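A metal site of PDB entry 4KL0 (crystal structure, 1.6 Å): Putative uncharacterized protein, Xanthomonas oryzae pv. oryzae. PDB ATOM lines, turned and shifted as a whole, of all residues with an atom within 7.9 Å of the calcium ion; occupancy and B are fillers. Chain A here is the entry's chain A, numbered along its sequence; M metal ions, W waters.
N of Asp 318 is in hydrogen-bond range of OD2 of Asp 41 (3.1 Å).
N of Ile 151 lies within hydrogen-bond range of O of Phe 33 (2.9 Å).
OD1 of Asp 42 sits close to OG1 of Thr 34, 2.6 Å away.
Of the 24 residues printed, 4 come within 4 Å of the calcium ion.
The nearest printed residue that does not touch the calcium ion is Lys 38 (4.4 Å).
The side-chain carboxylate (OD2) of Asp 318 is bound to the calcium ion, at 2.4 Å.
The calcium ion is bound by the backbone carbonyl oxygen (O) of Ile 151.
The calcium ion is bound by water W3, at 2.5 Å.
The side-chain carboxylate (OD1) of Asp 35 binds the calcium ion, at 2.5 Å.
OD2 of Asp 42 is bound to the calcium ion.
Water W2 is bound to the calcium ion (2.6 Å).
Water W1 is bound to the calcium ion, at 2.7 Å.
The calcium ion is bound by OD1 of Asp 42, 2.8 Å away.
Water W1 lies within hydrogen-bond range of OD1 of Asp 318 (2.5 Å) and ND2 of Asn 199 (2.9 Å).
Water W3 bridges the side-chain carboxylate (OD2) of Asp 39 (2.9 Å) and the side-chain amino group (NZ) of Lys 38 (3.0 Å).
Water W2 lies within hydrogen-bond range of OD2 of Asp 35, OD1 of Asn 199 and NZ of Lys 38.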
ATOM      1  N   PHE A  33       7.658 -22.592  13.688  1.00  0.00           N
ATOM      2  CA  PHE A  33       6.325 -22.863  14.220  1.00  0.00           C
ATOM      3  C   PHE A  33       5.521 -21.582  14.090  1.00  0.00           C
ATOM      4  O   PHE A  33       5.955 -20.544  14.585  1.00  0.00           O
ATOM      5  CB  PHE A  33       6.446 -23.275  15.698  1.00  0.00           C
ATOM      6  CG  PHE A  33       7.328 -24.468  15.894  1.00  0.00           C
ATOM      7  CD1 PHE A  33       6.760 -25.741  16.016  1.00  0.00           C
ATOM      8  CD2 PHE A  33       8.702 -24.303  15.972  1.00  0.00           C
ATOM      9  CE1 PHE A  33       7.629 -26.882  16.161  1.00  0.00           C
ATOM     10  CE2 PHE A  33       9.557 -25.437  16.112  1.00  0.00           C
ATOM     11  CZ  PHE A  33       8.954 -26.718  16.227  1.00  0.00           C
ATOM     12  N   THR A  34       4.418 -21.605  13.337  1.00  0.00           N
ATOM     13  CA  THR A  34       3.841 -20.356  12.793  1.00  0.00           C
ATOM     14  C   THR A  34       2.326 -20.443  12.571  1.00  0.00           C
ATOM     15  O   THR A  34       1.768 -21.538  12.555  1.00  0.00           O
ATOM     16  CB  THR A  34       4.541 -20.087  11.468  1.00  0.00           C
ATOM     17  OG1 THR A  34       4.041 -18.902  10.829  1.00  0.00           O
ATOM     18  CG2 THR A  34       4.382 -21.241  10.518  1.00  0.00           C
ATOM     19  N   ASP A  35       1.651 -19.289  12.537  1.00  0.00           N
ATOM     20  CA  ASP A  35       0.173 -19.219  12.454  1.00  0.00           C
ATOM     21  C   ASP A  35      -0.222 -18.126  11.467  1.00  0.00           C
ATOM     22  O   ASP A  35      -0.793 -17.121  11.839  1.00  0.00           O
ATOM     23  CB  ASP A  35      -0.450 -18.957  13.842  1.00  0.00           C
ATOM     24  CG  ASP A  35       0.118 -17.704  14.545  1.00  0.00           C
ATOM     25  OD1 ASP A  35       1.027 -17.031  13.985  1.00  0.00           O
ATOM     26  OD2 ASP A  35      -0.413 -17.355  15.650  1.00  0.00           O
ATOM     27  N   PRO A  36       0.072 -18.362  10.198  1.00  0.00           N
ATOM     28  CA  PRO A  36      -0.093 -17.241   9.213  1.00  0.00           C
ATOM     29  C   PRO A  36      -1.553 -16.908   8.870  1.00  0.00           C
ATOM     30  O   PRO A  36      -2.517 -17.698   9.068  1.00  0.00           O
ATOM     31  CB  PRO A  36       0.607 -17.793   7.967  1.00  0.00           C
ATOM     32  CG  PRO A  36       0.404 -19.327   8.054  1.00  0.00           C
ATOM     33  CD  PRO A  36       0.631 -19.580   9.574  1.00  0.00           C
ATOM     34  N   ASN A  37      -1.679 -15.709   8.304  1.00  0.00           N
ATOM     35  CA  ASN A  37      -2.949 -15.193   7.751  1.00  0.00           C
ATOM     36  C   ASN A  37      -3.998 -14.796   8.776  1.00  0.00           C
ATOM     37  O   ASN A  37      -5.189 -14.770   8.460  1.00  0.00           O
ATOM     38  CB  ASN A  37      -3.513 -16.107   6.675  1.00  0.00           C
ATOM     39  CG  ASN A  37      -4.378 -15.347   5.697  1.00  0.00           C
ATOM     40  OD1 ASN A  37      -3.998 -14.240   5.280  1.00  0.00           O
ATOM     41  ND2 ASN A  37      -5.544 -15.917   5.322  1.00  0.00           N
ATOM     42  N   LYS A  38      -3.599 -14.500  10.008  1.00  0.00           N
ATOM     43  CA  LYS A  38      -4.488 -13.703  10.853  1.00  0.00           C
ATOM     44  C   LYS A  38      -3.950 -12.279  11.002  1.00  0.00           C
ATOM     45  O   LYS A  38      -4.648 -11.371  11.499  1.00  0.00           O
ATOM     46  CB  LYS A  38      -4.800 -14.360  12.220  1.00  0.00           C
ATOM     47  CG  LYS A  38      -3.644 -14.908  13.041  1.00  0.00           C
ATOM     48  CD  LYS A  38      -2.930 -13.819  13.875  1.00  0.00           C
ATOM     49  CE  LYS A  38      -1.851 -14.463  14.833  1.00  0.00           C
ATOM     50  NZ  LYS A  38      -1.143 -13.349  15.566  1.00  0.00           N
ATOM     51  N   ASP A  39      -2.746 -12.069  10.512  1.00  0.00           N
ATOM     52  CA  ASP A  39      -2.118 -10.730  10.458  1.00  0.00           C
ATOM     53  C   ASP A  39      -0.965 -10.839   9.439  1.00  0.00           C
ATOM     54  O   ASP A  39      -0.750 -11.911   8.887  1.00  0.00           O
ATOM     55  CB  ASP A  39      -1.667 -10.277  11.847  1.00  0.00           C
ATOM     56  CG  ASP A  39      -0.634 -11.192  12.515  1.00  0.00           C
ATOM     57  OD1 ASP A  39       0.170 -11.878  11.836  1.00  0.00           O
ATOM     58  OD2 ASP A  39      -0.639 -11.191  13.792  1.00  0.00           O
ATOM     59  N   PRO A  40      -0.215  -9.755   9.154  1.00  0.00           N
ATOM     60  CA  PRO A  40       0.856  -9.903   8.163  1.00  0.00           C
ATOM     61  C   PRO A  40       2.122 -10.574   8.620  1.00  0.00           C
ATOM     62  O   PRO A  40       2.916 -10.984   7.774  1.00  0.00           O
ATOM     63  CB  PRO A  40       1.229  -8.438   7.802  1.00  0.00           C
ATOM     64  CG  PRO A  40       0.170  -7.555   8.480  1.00  0.00           C
ATOM     65  CD  PRO A  40      -0.392  -8.362   9.617  1.00  0.00           C
ATOM     66  N   ASP A  41       2.315 -10.682   9.926  1.00  0.00           N
ATOM     67  CA  ASP A  41       3.649 -10.936  10.511  1.00  0.00           C
ATOM     68  C   ASP A  41       4.323 -12.200  10.034  1.00  0.00           C
ATOM     69  O   ASP A  41       5.512 -12.194   9.720  1.00  0.00           O
ATOM     70  CB  ASP A  41       3.481 -11.115  11.999  1.00  0.00           C
ATOM     71  CG  ASP A  41       3.477  -9.851  12.698  1.00  0.00           C
ATOM     72  OD1 ASP A  41       2.432  -9.128  12.638  1.00  0.00           O
ATOM     73  OD2 ASP A  41       4.519  -9.611  13.357  1.00  0.00           O
ATOM     74  N   ASP A  42       3.595 -13.325  10.063  1.00  0.00           N
ATOM     75  CA  ASP A  42       4.250 -14.583   9.710  1.00  0.00           C
ATOM     76  C   ASP A  42       4.700 -14.558   8.276  1.00  0.00           C
ATOM     77  O   ASP A  42       5.783 -15.088   7.961  1.00  0.00           O
ATOM     78  CB  ASP A  42       3.314 -15.778  10.016  1.00  0.00           C
ATOM     79  CG  ASP A  42       2.909 -15.835  11.487  1.00  0.00           C
ATOM     80  OD1 ASP A  42       3.413 -16.741  12.159  1.00  0.00           O
ATOM     81  OD2 ASP A  42       2.089 -14.965  11.959  1.00  0.00           O
ATOM     82  N   VAL A  43       3.860 -14.007   7.392  1.00  0.00           N
ATOM     83  CA  VAL A  43       4.249 -14.006   5.971  1.00  0.00           C
ATOM     84  C   VAL A  43       5.379 -13.037   5.666  1.00  0.00           C
ATOM     85  O   VAL A  43       6.218 -13.356   4.810  1.00  0.00           O
ATOM     86  CB  VAL A  43       3.017 -13.790   5.097  1.00  0.00           C
ATOM     87  CG1 VAL A  43       3.441 -13.555   3.616  1.00  0.00           C
ATOM     88  CG2 VAL A  43       2.135 -15.065   5.219  1.00  0.00           C
ATOM     89  N   THR A  45       7.733 -12.755   7.738  1.00  0.00           N
ATOM     90  CA  THR A  45       8.862 -13.577   8.194  1.00  0.00           C
ATOM     91  C   THR A  45       9.272 -14.567   7.109  1.00  0.00           C
ATOM     92  O   THR A  45      10.475 -14.798   6.902  1.00  0.00           O
ATOM     93  CB  THR A  45       8.468 -14.352   9.484  1.00  0.00           C
ATOM     94  OG1 THR A  45       7.951 -13.429  10.424  1.00  0.00           O
ATOM     95  CG2 THR A  45       9.684 -15.060  10.074  1.00  0.00           C
ATOM     96  N   TYR A  46       8.299 -15.200   6.420  1.00  0.00           N
ATOM     97  CA  TYR A  46       8.639 -16.158   5.367  1.00  0.00           C
ATOM     98  C   TYR A  46       9.415 -15.415   4.278  1.00  0.00           C
ATOM     99  O   TYR A  46      10.381 -15.948   3.681  1.00  0.00           O
ATOM    100  CB  TYR A  46       7.389 -16.769   4.717  1.00  0.00           C
ATOM    101  CG  TYR A  46       6.403 -17.440   5.643  1.00  0.00           C
ATOM    102  CD1 TYR A  46       6.780 -17.845   6.929  1.00  0.00           C
ATOM    103  CD2 TYR A  46       5.113 -17.671   5.248  1.00  0.00           C
ATOM    104  CE1 TYR A  46       5.840 -18.427   7.799  1.00  0.00           C
ATOM    105  CE2 TYR A  46       4.199 -18.273   6.075  1.00  0.00           C
ATOM    106  CZ  TYR A  46       4.552 -18.651   7.352  1.00  0.00           C
ATOM    107  OH  TYR A  46       3.581 -19.194   8.151  1.00  0.00           O
ATOM    108  N   LEU A  67      -2.927 -22.745  15.260  1.00  0.00           N
ATOM    109  CA  LEU A  67      -3.985 -21.743  15.494  1.00  0.00           C
ATOM    110  C   LEU A  67      -5.264 -22.102  14.727  1.00  0.00           C
ATOM    111  O   LEU A  67      -5.303 -21.997  13.487  1.00  0.00           O
ATOM    112  CB  LEU A  67      -3.549 -20.277  15.163  1.00  0.00           C
ATOM    113  CG  LEU A  67      -4.518 -19.211  15.653  1.00  0.00           C
ATOM    114  CD1 LEU A  67      -4.401 -19.030  17.202  1.00  0.00           C
ATOM    115  CD2 LEU A  67      -4.072 -17.897  15.010  1.00  0.00           C
ATOM    116  N   VAL A 150       9.998 -19.835  17.121  1.00  0.00           N
ATOM    117  CA  VAL A 150       8.557 -19.942  17.470  1.00  0.00           C
ATOM    118  C   VAL A 150       7.910 -18.598  17.316  1.00  0.00           C
ATOM    119  O   VAL A 150       8.241 -17.650  18.031  1.00  0.00           O
ATOM    120  CB  VAL A 150       8.402 -20.466  18.904  1.00  0.00           C
ATOM    121  CG1 VAL A 150       6.939 -20.482  19.323  1.00  0.00           C
ATOM    122  CG2 VAL A 150       9.137 -21.821  19.040  1.00  0.00           C
ATOM    123  N   ILE A 151       6.989 -18.487  16.346  1.00  0.00           N
ATOM    124  CA  ILE A 151       6.299 -17.222  16.117  1.00  0.00           C
ATOM    125  C   ILE A 151       4.804 -17.478  16.153  1.00  0.00           C
ATOM    126  O   ILE A 151       4.082 -16.764  15.509  1.00  0.00           O
ATOM    127  CB  ILE A 151       6.719 -16.574  14.775  1.00  0.00           C
ATOM    128  CG1 ILE A 151       6.632 -17.552  13.583  1.00  0.00           C
ATOM    129  CG2 ILE A 151       8.198 -16.088  14.900  1.00  0.00           C
ATOM    130  CD1 ILE A 151       6.889 -16.913  12.236  1.00  0.00           C
ATOM    131  N   ALA A 152       4.376 -18.404  16.990  1.00  0.00           N
ATOM    132  CA  ALA A 152       2.963 -18.733  17.191  1.00  0.00           C
ATOM    133  C   ALA A 152       2.821 -19.515  18.456  1.00  0.00           C
ATOM    134  O   ALA A 152       3.810 -19.631  19.165  1.00  0.00           O
ATOM    135  CB  ALA A 152       2.406 -19.610  15.993  1.00  0.00           C
ATOM    136  N   GLY A 153       1.636 -20.111  18.684  1.00  0.00           N
ATOM    137  CA  GLY A 153       1.408 -20.925  19.884  1.00  0.00           C
ATOM    138  C   GLY A 153       2.315 -22.133  19.852  1.00  0.00           C
ATOM    139  O   GLY A 153       2.869 -22.554  18.801  1.00  0.00           O
ATOM    140  N   MET A 178       8.725 -15.504  20.039  1.00  0.00           N
ATOM    141  CA  MET A 178       8.063 -14.219  20.122  1.00  0.00           C
ATOM    142  C   MET A 178       7.032 -14.405  21.225  1.00  0.00           C
ATOM    143  O   MET A 178       5.983 -15.042  21.041  1.00  0.00           O
ATOM    144  CB  MET A 178       7.376 -13.930  18.749  1.00  0.00           C
ATOM    145  CG  MET A 178       6.918 -12.484  18.532  1.00  0.00           C
ATOM    146  SD  MET A 178       5.472 -11.903  19.564  1.00  0.00           S
ATOM    147  CE  MET A 178       6.370 -10.620  20.511  1.00  0.00           C
ATOM    148  N   TYR A 198       0.467 -12.956  23.514  1.00  0.00           N
ATOM    149  CA  TYR A 198      -0.443 -13.616  22.566  1.00  0.00           C
ATOM    150  C   TYR A 198      -0.044 -15.062  22.258  1.00  0.00           C
ATOM    151  O   TYR A 198      -0.870 -16.002  22.357  1.00  0.00           O
ATOM    152  CB  TYR A 198      -0.512 -12.795  21.250  1.00  0.00           C
ATOM    153  CG  TYR A 198      -1.502 -13.374  20.236  1.00  0.00           C
ATOM    154  CD1 TYR A 198      -2.806 -12.886  20.133  1.00  0.00           C
ATOM    155  CD2 TYR A 198      -1.116 -14.412  19.389  1.00  0.00           C
ATOM    156  CE1 TYR A 198      -3.720 -13.426  19.219  1.00  0.00           C
ATOM    157  CE2 TYR A 198      -2.006 -14.973  18.496  1.00  0.00           C
ATOM    158  CZ  TYR A 198      -3.312 -14.478  18.405  1.00  0.00           C
ATOM    159  OH  TYR A 198      -4.192 -15.056  17.498  1.00  0.00           O
ATOM    160  N   ASN A 199       1.217 -15.256  21.894  1.00  0.00           N
ATOM    161  CA  ASN A 199       1.635 -16.605  21.506  1.00  0.00           C
ATOM    162  C   ASN A 199       1.623 -17.580  22.676  1.00  0.00           C
ATOM    163  O   ASN A 199       1.409 -18.759  22.533  1.00  0.00           O
ATOM    164  CB  ASN A 199       2.974 -16.653  20.819  1.00  0.00           C
ATOM    165  CG  ASN A 199       2.891 -16.013  19.419  1.00  0.00           C
ATOM    166  OD1 ASN A 199       1.792 -16.058  18.798  1.00  0.00           O
ATOM    167  ND2 ASN A 199       3.972 -15.380  18.962  1.00  0.00           N
ATOM    168  N   TYR A 317       6.599  -8.127  14.622  1.00  0.00           N
ATOM    169  CA  TYR A 317       7.089  -8.900  15.743  1.00  0.00           C
ATOM    170  C   TYR A 317       7.802 -10.145  15.293  1.00  0.00           C
ATOM    171  O   TYR A 317       8.878 -10.469  15.759  1.00  0.00           O
ATOM    172  CB  TYR A 317       5.905  -9.368  16.623  1.00  0.00           C
ATOM    173  CG  TYR A 317       4.962  -8.262  17.032  1.00  0.00           C
ATOM    174  CD1 TYR A 317       5.248  -7.457  18.110  1.00  0.00           C
ATOM    175  CD2 TYR A 317       3.776  -8.060  16.338  1.00  0.00           C
ATOM    176  CE1 TYR A 317       4.374  -6.431  18.504  1.00  0.00           C
ATOM    177  CE2 TYR A 317       2.889  -7.040  16.701  1.00  0.00           C
ATOM    178  CZ  TYR A 317       3.198  -6.244  17.778  1.00  0.00           C
ATOM    179  OH  TYR A 317       2.319  -5.237  18.157  1.00  0.00           O
ATOM    180  N   ASP A 318       7.198 -10.858  14.373  1.00  0.00           N
ATOM    181  CA  ASP A 318       7.762 -12.129  13.992  1.00  0.00           C
ATOM    182  C   ASP A 318       9.056 -12.013  13.153  1.00  0.00           C
ATOM    183  O   ASP A 318      10.006 -12.807  13.335  1.00  0.00           O
ATOM    184  CB  ASP A 318       6.703 -12.970  13.273  1.00  0.00           C
ATOM    185  CG  ASP A 318       5.585 -13.401  14.189  1.00  0.00           C
ATOM    186  OD1 ASP A 318       5.691 -13.262  15.423  1.00  0.00           O
ATOM    187  OD2 ASP A 318       4.562 -13.947  13.721  1.00  0.00           O
ATOM    188  N   PRO A 319       9.126 -11.050  12.226  1.00  0.00           N
ATOM    189  CA  PRO A 319      10.379 -10.923  11.481  1.00  0.00           C
ATOM    190  C   PRO A 319      11.516 -10.562  12.415  1.00  0.00           C
ATOM    191  O   PRO A 319      12.615 -11.084  12.218  1.00  0.00           O
ATOM    192  CB  PRO A 319      10.095  -9.727  10.580  1.00  0.00           C
ATOM    193  CG  PRO A 319       8.662  -9.873  10.270  1.00  0.00           C
ATOM    194  CD  PRO A 319       8.027 -10.298  11.586  1.00  0.00           C
HETATM  195 CA    CA M   1       2.648 -15.185  14.376  1.00  0.00          CA
HETATM  196  O   HOH W   1       3.481 -13.814  16.540  1.00  0.00           O
HETATM  197  O   HOH W   2       0.947 -15.299  16.345  1.00  0.00           O
HETATM  198  O   HOH W   3       1.522 -12.968  14.346  1.00  0.00           O
